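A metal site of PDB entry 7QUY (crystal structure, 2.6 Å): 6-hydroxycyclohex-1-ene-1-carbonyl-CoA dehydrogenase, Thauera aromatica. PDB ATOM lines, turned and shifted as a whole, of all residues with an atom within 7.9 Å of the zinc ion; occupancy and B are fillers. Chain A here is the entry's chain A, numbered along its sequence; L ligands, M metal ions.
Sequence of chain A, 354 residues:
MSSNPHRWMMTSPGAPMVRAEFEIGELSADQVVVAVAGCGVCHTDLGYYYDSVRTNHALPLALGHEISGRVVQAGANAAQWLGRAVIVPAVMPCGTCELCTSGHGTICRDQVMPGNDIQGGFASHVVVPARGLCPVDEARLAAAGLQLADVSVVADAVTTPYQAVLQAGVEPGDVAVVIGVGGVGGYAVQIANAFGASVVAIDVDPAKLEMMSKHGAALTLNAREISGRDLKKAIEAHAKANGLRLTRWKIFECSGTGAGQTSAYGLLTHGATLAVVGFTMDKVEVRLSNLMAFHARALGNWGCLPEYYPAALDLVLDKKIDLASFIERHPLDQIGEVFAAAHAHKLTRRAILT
An oxygen (O9) of the ligand lies within hydrogen-bond range of the backbone NH (N) of Val 184 (2.8 Å).
ND1 of His 65 lies within hydrogen-bond range of OD1 of Asp 45 (3.5 Å).
The side-chain carboxylate (OE2) of Glu 66 lies close to the side-chain sulfur (SG) of Cys 42 (3.5 Å).
The side-chain carboxylate (OE1) of Glu 66 is in salt-bridge range of the guanidinium group (NE) of Arg 350.
The backbone carbonyl oxygen (O) of Glu 66 lies within hydrogen-bond range of the backbone NH (N) of Gly 40 (2.8 Å).
The side-chain sulfur (SG) of Cys 42 lies close to the side-chain carboxylate (OD2) of Asp 156 (3.6 Å).
The side-chain hydroxyl of Thr 160 is in hydrogen-bond range of the side-chain carboxylate of Asp 156 (2.8 Å).
NH2 of Arg 350 lies within hydrogen-bond range of SG of Cys 42 (3.3 Å).
The backbone NH of Thr 44 sits close to the side-chain sulfur of Cys 42, 3.5 Å away.
Merely in contact with the zinc ion: Arg 350 (3.97 Å).
Of the 18 residues printed, 5 come within 4 Å of the zinc ion.
The zinc ion is bound by a ring nitrogen (NE2) of His 65 (2.0 Å), the side-chain carboxylate of Glu 66 (2.0 Å) and the side-chain carboxylate of Asp 156 (2.0 Å).
The zinc ion has three donor atoms within binding distance.
Slightly farther from the zinc ion lies the side-chain sulfur (SG) of Cys 42 (2.8 Å).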
ATOM      1  N   GLY A  40     -30.597 -11.513 -19.610  1.00  0.00           N
ATOM      2  CA  GLY A  40     -30.307 -10.988 -18.270  1.00  0.00           C
ATOM      3  C   GLY A  40     -29.608  -9.641 -18.360  1.00  0.00           C
ATOM      4  O   GLY A  40     -28.882  -9.412 -19.346  1.00  0.00           O
ATOM      5  N   VAL A  41     -29.784  -8.818 -17.317  1.00  0.00           N
ATOM      6  CA  VAL A  41     -29.093  -7.525 -17.107  1.00  0.00           C
ATOM      7  C   VAL A  41     -28.036  -7.712 -16.017  1.00  0.00           C
ATOM      8  O   VAL A  41     -28.393  -7.988 -14.857  1.00  0.00           O
ATOM      9  CB  VAL A  41     -30.089  -6.433 -16.693  1.00  0.00           C
ATOM     10  CG1 VAL A  41     -29.399  -5.128 -16.374  1.00  0.00           C
ATOM     11  CG2 VAL A  41     -31.175  -6.239 -17.749  1.00  0.00           C
ATOM     12  N   CYS A  42     -26.771  -7.568 -16.434  1.00  0.00           N
ATOM     13  CA  CYS A  42     -25.648  -7.834 -15.506  1.00  0.00           C
ATOM     14  C   CYS A  42     -24.878  -6.553 -15.164  1.00  0.00           C
ATOM     15  O   CYS A  42     -25.040  -5.547 -15.880  1.00  0.00           O
ATOM     16  CB  CYS A  42     -24.672  -8.814 -16.147  1.00  0.00           C
ATOM     17  SG  CYS A  42     -23.294  -9.292 -15.074  1.00  0.00           S
ATOM     18  N   HIS A  43     -24.062  -6.611 -14.115  1.00  0.00           N
ATOM     19  CA  HIS A  43     -23.223  -5.480 -13.660  1.00  0.00           C
ATOM     20  C   HIS A  43     -22.219  -5.174 -14.776  1.00  0.00           C
ATOM     21  O   HIS A  43     -21.813  -4.011 -14.901  1.00  0.00           O
ATOM     22  CB  HIS A  43     -22.594  -5.761 -12.279  1.00  0.00           C
ATOM     23  CG  HIS A  43     -23.515  -5.418 -11.157  1.00  0.00           C
ATOM     24  ND1 HIS A  43     -23.199  -4.479 -10.180  1.00  0.00           N
ATOM     25  CD2 HIS A  43     -24.767  -5.857 -10.858  1.00  0.00           C
ATOM     26  CE1 HIS A  43     -24.209  -4.379  -9.329  1.00  0.00           C
ATOM     27  NE2 HIS A  43     -25.180  -5.206  -9.733  1.00  0.00           N
ATOM     28  N   THR A  44     -21.870  -6.173 -15.587  1.00  0.00           N
ATOM     29  CA  THR A  44     -20.975  -6.012 -16.758  1.00  0.00           C
ATOM     30  C   THR A  44     -21.664  -5.049 -17.743  1.00  0.00           C
ATOM     31  O   THR A  44     -20.948  -4.170 -18.270  1.00  0.00           O
ATOM     32  CB  THR A  44     -20.676  -7.361 -17.421  1.00  0.00           C
ATOM     33  OG1 THR A  44     -20.211  -8.266 -16.426  1.00  0.00           O
ATOM     34  CG2 THR A  44     -19.586  -7.285 -18.459  1.00  0.00           C
ATOM     35  N   ASP A  45     -22.968  -5.227 -17.979  1.00  0.00           N
ATOM     36  CA  ASP A  45     -23.784  -4.386 -18.897  1.00  0.00           C
ATOM     37  C   ASP A  45     -23.865  -2.971 -18.320  1.00  0.00           C
ATOM     38  O   ASP A  45     -23.576  -2.003 -19.053  1.00  0.00           O
ATOM     39  CB  ASP A  45     -25.147  -5.017 -19.138  1.00  0.00           C
ATOM     40  CG  ASP A  45     -25.109  -6.340 -19.877  1.00  0.00           C
ATOM     41  OD1 ASP A  45     -24.354  -6.437 -20.863  1.00  0.00           O
ATOM     42  OD2 ASP A  45     -25.830  -7.274 -19.457  1.00  0.00           O
ATOM     43  N   GLY A  64     -25.983  -7.241 -23.635  1.00  0.00           N
ATOM     44  CA  GLY A  64     -26.723  -8.449 -23.222  1.00  0.00           C
ATOM     45  C   GLY A  64     -26.003  -9.711 -23.691  1.00  0.00           C
ATOM     46  O   GLY A  64     -25.911  -9.943 -24.920  1.00  0.00           O
ATOM     47  N   HIS A  65     -25.507 -10.486 -22.732  1.00  0.00           N
ATOM     48  CA  HIS A  65     -24.739 -11.743 -22.924  1.00  0.00           C
ATOM     49  C   HIS A  65     -25.423 -12.919 -22.198  1.00  0.00           C
ATOM     50  O   HIS A  65     -25.020 -14.087 -22.427  1.00  0.00           O
ATOM     51  CB  HIS A  65     -23.301 -11.507 -22.499  1.00  0.00           C
ATOM     52  CG  HIS A  65     -23.178 -11.008 -21.102  1.00  0.00           C
ATOM     53  ND1 HIS A  65     -23.058  -9.658 -20.799  1.00  0.00           N
ATOM     54  CD2 HIS A  65     -23.135 -11.666 -19.935  1.00  0.00           C
ATOM     55  CE1 HIS A  65     -22.945  -9.525 -19.492  1.00  0.00           C
ATOM     56  NE2 HIS A  65     -22.990 -10.759 -18.938  1.00  0.00           N
ATOM     57  N   GLU A  66     -26.479 -12.654 -21.435  1.00  0.00           N
ATOM     58  CA  GLU A  66     -27.184 -13.672 -20.635  1.00  0.00           C
ATOM     59  C   GLU A  66     -28.462 -14.080 -21.399  1.00  0.00           C
ATOM     60  O   GLU A  66     -29.550 -13.679 -20.963  1.00  0.00           O
ATOM     61  CB  GLU A  66     -27.402 -13.125 -19.223  1.00  0.00           C
ATOM     62  CG  GLU A  66     -26.103 -12.821 -18.471  1.00  0.00           C
ATOM     63  CD  GLU A  66     -26.263 -12.303 -17.033  1.00  0.00           C
ATOM     64  OE1 GLU A  66     -27.396 -12.386 -16.461  1.00  0.00           O
ATOM     65  OE2 GLU A  66     -25.286 -11.795 -16.493  1.00  0.00           O
ATOM     66  N   ALA A  90     -22.322 -17.081 -22.649  1.00  0.00           N
ATOM     67  CA  ALA A  90     -21.938 -15.671 -22.480  1.00  0.00           C
ATOM     68  C   ALA A  90     -20.629 -15.394 -23.222  1.00  0.00           C
ATOM     69  O   ALA A  90     -20.436 -14.235 -23.659  1.00  0.00           O
ATOM     70  CB  ALA A  90     -21.807 -15.354 -21.005  1.00  0.00           C
ATOM     71  N   MET A 113     -17.934 -12.811 -27.144  1.00  0.00           N
ATOM     72  CA  MET A 113     -18.985 -12.537 -26.135  1.00  0.00           C
ATOM     73  C   MET A 113     -20.068 -11.685 -26.789  1.00  0.00           C
ATOM     74  O   MET A 113     -19.821 -10.575 -27.231  1.00  0.00           O
ATOM     75  CB  MET A 113     -18.351 -11.780 -24.970  1.00  0.00           C
ATOM     76  CG  MET A 113     -19.312 -11.128 -24.015  1.00  0.00           C
ATOM     77  SD  MET A 113     -18.339 -10.508 -22.597  1.00  0.00           S
ATOM     78  CE  MET A 113     -19.658  -9.696 -21.692  1.00  0.00           C
ATOM     79  N   VAL A 153     -30.444 -16.312 -17.464  1.00  0.00           N
ATOM     80  CA  VAL A 153     -29.412 -15.943 -16.443  1.00  0.00           C
ATOM     81  C   VAL A 153     -28.549 -17.148 -16.046  1.00  0.00           C
ATOM     82  O   VAL A 153     -27.587 -16.928 -15.289  1.00  0.00           O
ATOM     83  CB  VAL A 153     -30.055 -15.339 -15.185  1.00  0.00           C
ATOM     84  CG1 VAL A 153     -30.781 -14.036 -15.490  1.00  0.00           C
ATOM     85  CG2 VAL A 153     -30.990 -16.327 -14.525  1.00  0.00           C
ATOM     86  N   ALA A 155     -26.550 -18.452 -18.070  1.00  0.00           N
ATOM     87  CA  ALA A 155     -25.345 -17.853 -18.690  1.00  0.00           C
ATOM     88  C   ALA A 155     -24.765 -16.790 -17.758  1.00  0.00           C
ATOM     89  O   ALA A 155     -25.520 -15.897 -17.327  1.00  0.00           O
ATOM     90  CB  ALA A 155     -25.698 -17.290 -20.039  1.00  0.00           C
ATOM     91  N   ASP A 156     -23.456 -16.870 -17.504  1.00  0.00           N
ATOM     92  CA  ASP A 156     -22.668 -15.990 -16.596  1.00  0.00           C
ATOM     93  C   ASP A 156     -23.113 -16.212 -15.141  1.00  0.00           C
ATOM     94  O   ASP A 156     -22.336 -16.815 -14.381  1.00  0.00           O
ATOM     95  CB  ASP A 156     -22.718 -14.531 -17.044  1.00  0.00           C
ATOM     96  CG  ASP A 156     -21.719 -13.652 -16.298  1.00  0.00           C
ATOM     97  OD1 ASP A 156     -20.767 -14.197 -15.707  1.00  0.00           O
ATOM     98  OD2 ASP A 156     -21.897 -12.411 -16.314  1.00  0.00           O
ATOM     99  N   ALA A 157     -24.311 -15.747 -14.746  1.00  0.00           N
ATOM    100  CA  ALA A 157     -24.735 -15.643 -13.329  1.00  0.00           C
ATOM    101  C   ALA A 157     -24.635 -17.003 -12.613  1.00  0.00           C
ATOM    102  O   ALA A 157     -24.180 -17.039 -11.441  1.00  0.00           O
ATOM    103  CB  ALA A 157     -26.146 -15.100 -13.228  1.00  0.00           C
ATOM    104  N   THR A 160     -20.701 -18.985 -14.039  1.00  0.00           N
ATOM    105  CA  THR A 160     -19.446 -18.389 -13.520  1.00  0.00           C
ATOM    106  C   THR A 160     -19.138 -19.031 -12.164  1.00  0.00           C
ATOM    107  O   THR A 160     -18.112 -19.696 -12.023  1.00  0.00           O
ATOM    108  CB  THR A 160     -19.513 -16.849 -13.553  1.00  0.00           C
ATOM    109  OG1 THR A 160     -19.358 -16.515 -14.940  1.00  0.00           O
ATOM    110  CG2 THR A 160     -18.458 -16.166 -12.704  1.00  0.00           C
ATOM    111  N   VAL A 184     -23.609 -13.397  -8.462  1.00  0.00           N
ATOM    112  CA  VAL A 184     -22.711 -14.584  -8.597  1.00  0.00           C
ATOM    113  C   VAL A 184     -22.665 -15.337  -7.258  1.00  0.00           C
ATOM    114  O   VAL A 184     -22.896 -16.567  -7.274  1.00  0.00           O
ATOM    115  CB  VAL A 184     -21.331 -14.092  -9.042  1.00  0.00           C
ATOM    116  CG1 VAL A 184     -20.234 -15.118  -8.769  1.00  0.00           C
ATOM    117  CG2 VAL A 184     -21.361 -13.680 -10.500  1.00  0.00           C
ATOM    118  N   ARG A 350     -32.739 -10.316 -10.141  1.00  0.00           N
ATOM    119  CA  ARG A 350     -31.969 -10.095 -11.386  1.00  0.00           C
ATOM    120  C   ARG A 350     -32.996  -9.859 -12.506  1.00  0.00           C
ATOM    121  O   ARG A 350     -33.932 -10.661 -12.618  1.00  0.00           O
ATOM    122  CB  ARG A 350     -31.045 -11.291 -11.683  1.00  0.00           C
ATOM    123  CG  ARG A 350     -29.985 -11.027 -12.744  1.00  0.00           C
ATOM    124  CD  ARG A 350     -29.108 -12.229 -13.018  1.00  0.00           C
ATOM    125  NE  ARG A 350     -27.880 -11.887 -13.717  1.00  0.00           N
ATOM    126  CZ  ARG A 350     -26.821 -11.309 -13.164  1.00  0.00           C
ATOM    127  NH1 ARG A 350     -26.821 -11.042 -11.875  1.00  0.00           N
ATOM    128  NH2 ARG A 350     -25.756 -11.052 -13.884  1.00  0.00           N
HETATM  129  P1  LIG L   1     -23.192  -8.011  -6.589  1.00  0.00           P
HETATM  130  O1  LIG L   1     -23.115  -6.528  -6.379  1.00  0.00           O
HETATM  131  O2  LIG L   1     -24.470  -8.640  -7.038  1.00  0.00           O
HETATM  132  O3  LIG L   1     -22.683  -8.753  -5.259  1.00  0.00           O
HETATM  133  C1  LIG L   1     -21.552  -8.334  -4.460  1.00  0.00           C
HETATM  134  C2  LIG L   1     -21.858  -8.706  -3.027  1.00  0.00           C
HETATM  135  O4  LIG L   1     -20.713  -8.423  -2.186  1.00  0.00           O
HETATM  136  C3  LIG L   1     -23.049  -7.960  -2.388  1.00  0.00           C
HETATM  137  O5  LIG L   1     -23.968  -8.899  -1.858  1.00  0.00           O
HETATM  138  C4  LIG L   1     -22.370  -7.038  -1.359  1.00  0.00           C
HETATM  139  O6  LIG L   1     -23.167  -6.683  -0.254  1.00  0.00           O
HETATM  140  C5  LIG L   1     -21.217  -7.942  -0.959  1.00  0.00           C
HETATM  141  N1  LIG L   1     -20.129  -7.296  -0.241  1.00  0.00           N
HETATM  142  C6  LIG L   1     -19.589  -6.061  -0.505  1.00  0.00           C
HETATM  143  N2  LIG L   1     -18.585  -5.774   0.274  1.00  0.00           N
HETATM  144  C7  LIG L   1     -18.418  -6.889   1.084  1.00  0.00           C
HETATM  145  C8  LIG L   1     -17.504  -7.208   2.112  1.00  0.00           C
HETATM  146  N3  LIG L   1     -16.540  -6.381   2.494  1.00  0.00           N
HETATM  147  N4  LIG L   1     -17.594  -8.423   2.711  1.00  0.00           N
HETATM  148  C9  LIG L   1     -18.577  -9.231   2.297  1.00  0.00           C
HETATM  149  N5  LIG L   1     -19.504  -9.032   1.350  1.00  0.00           N
HETATM  150  C10 LIG L   1     -19.370  -7.837   0.764  1.00  0.00           C
HETATM  151  O7  LIG L   1     -22.069  -8.475  -7.633  1.00  0.00           O
HETATM  152  P2  LIG L   1     -22.030  -9.733  -8.638  1.00  0.00           P
HETATM  153  O8  LIG L   1     -22.979  -9.491  -9.754  1.00  0.00           O
HETATM  154  O9  LIG L   1     -22.211 -11.008  -7.906  1.00  0.00           O
HETATM  155  O10 LIG L   1     -20.492  -9.618  -9.088  1.00  0.00           O
HETATM  156  C11 LIG L   1     -19.539  -9.617  -7.990  1.00  0.00           C
HETATM  157  C12 LIG L   1     -18.133  -9.705  -8.529  1.00  0.00           C
HETATM  158  O11 LIG L   1     -18.057 -10.793  -9.482  1.00  0.00           O
HETATM  159  C13 LIG L   1     -17.640  -8.457  -9.280  1.00  0.00           C
HETATM  160  O12 LIG L   1     -16.316  -8.097  -8.900  1.00  0.00           O
HETATM  161  C14 LIG L   1     -17.767  -8.905 -10.742  1.00  0.00           C
HETATM  162  O13 LIG L   1     -16.971  -8.079 -11.584  1.00  0.00           O
HETATM  163  C15 LIG L   1     -17.316 -10.362 -10.612  1.00  0.00           C
HETATM  164  N6  LIG L   1     -17.644 -11.246 -11.765  1.00  0.00           N
HETATM  165  C16 LIG L   1     -16.643 -11.952 -12.378  1.00  0.00           C
HETATM  166  C17 LIG L   1     -16.927 -12.989 -13.251  1.00  0.00           C
HETATM  167  C18 LIG L   1     -15.853 -14.024 -13.508  1.00  0.00           C
HETATM  168  O14 LIG L   1     -15.772 -14.561 -14.622  1.00  0.00           O
HETATM  169  N7  LIG L   1     -15.024 -14.323 -12.515  1.00  0.00           N
HETATM  170  C19 LIG L   1     -18.187 -13.020 -13.818  1.00  0.00           C
HETATM  171  C20 LIG L   1     -19.194 -12.219 -13.295  1.00  0.00           C
HETATM  172  C21 LIG L   1     -18.913 -11.391 -12.214  1.00  0.00           C
HETATM  173 ZN    ZN M   1     -23.419 -11.286 -17.088  1.00  0.00          ZN
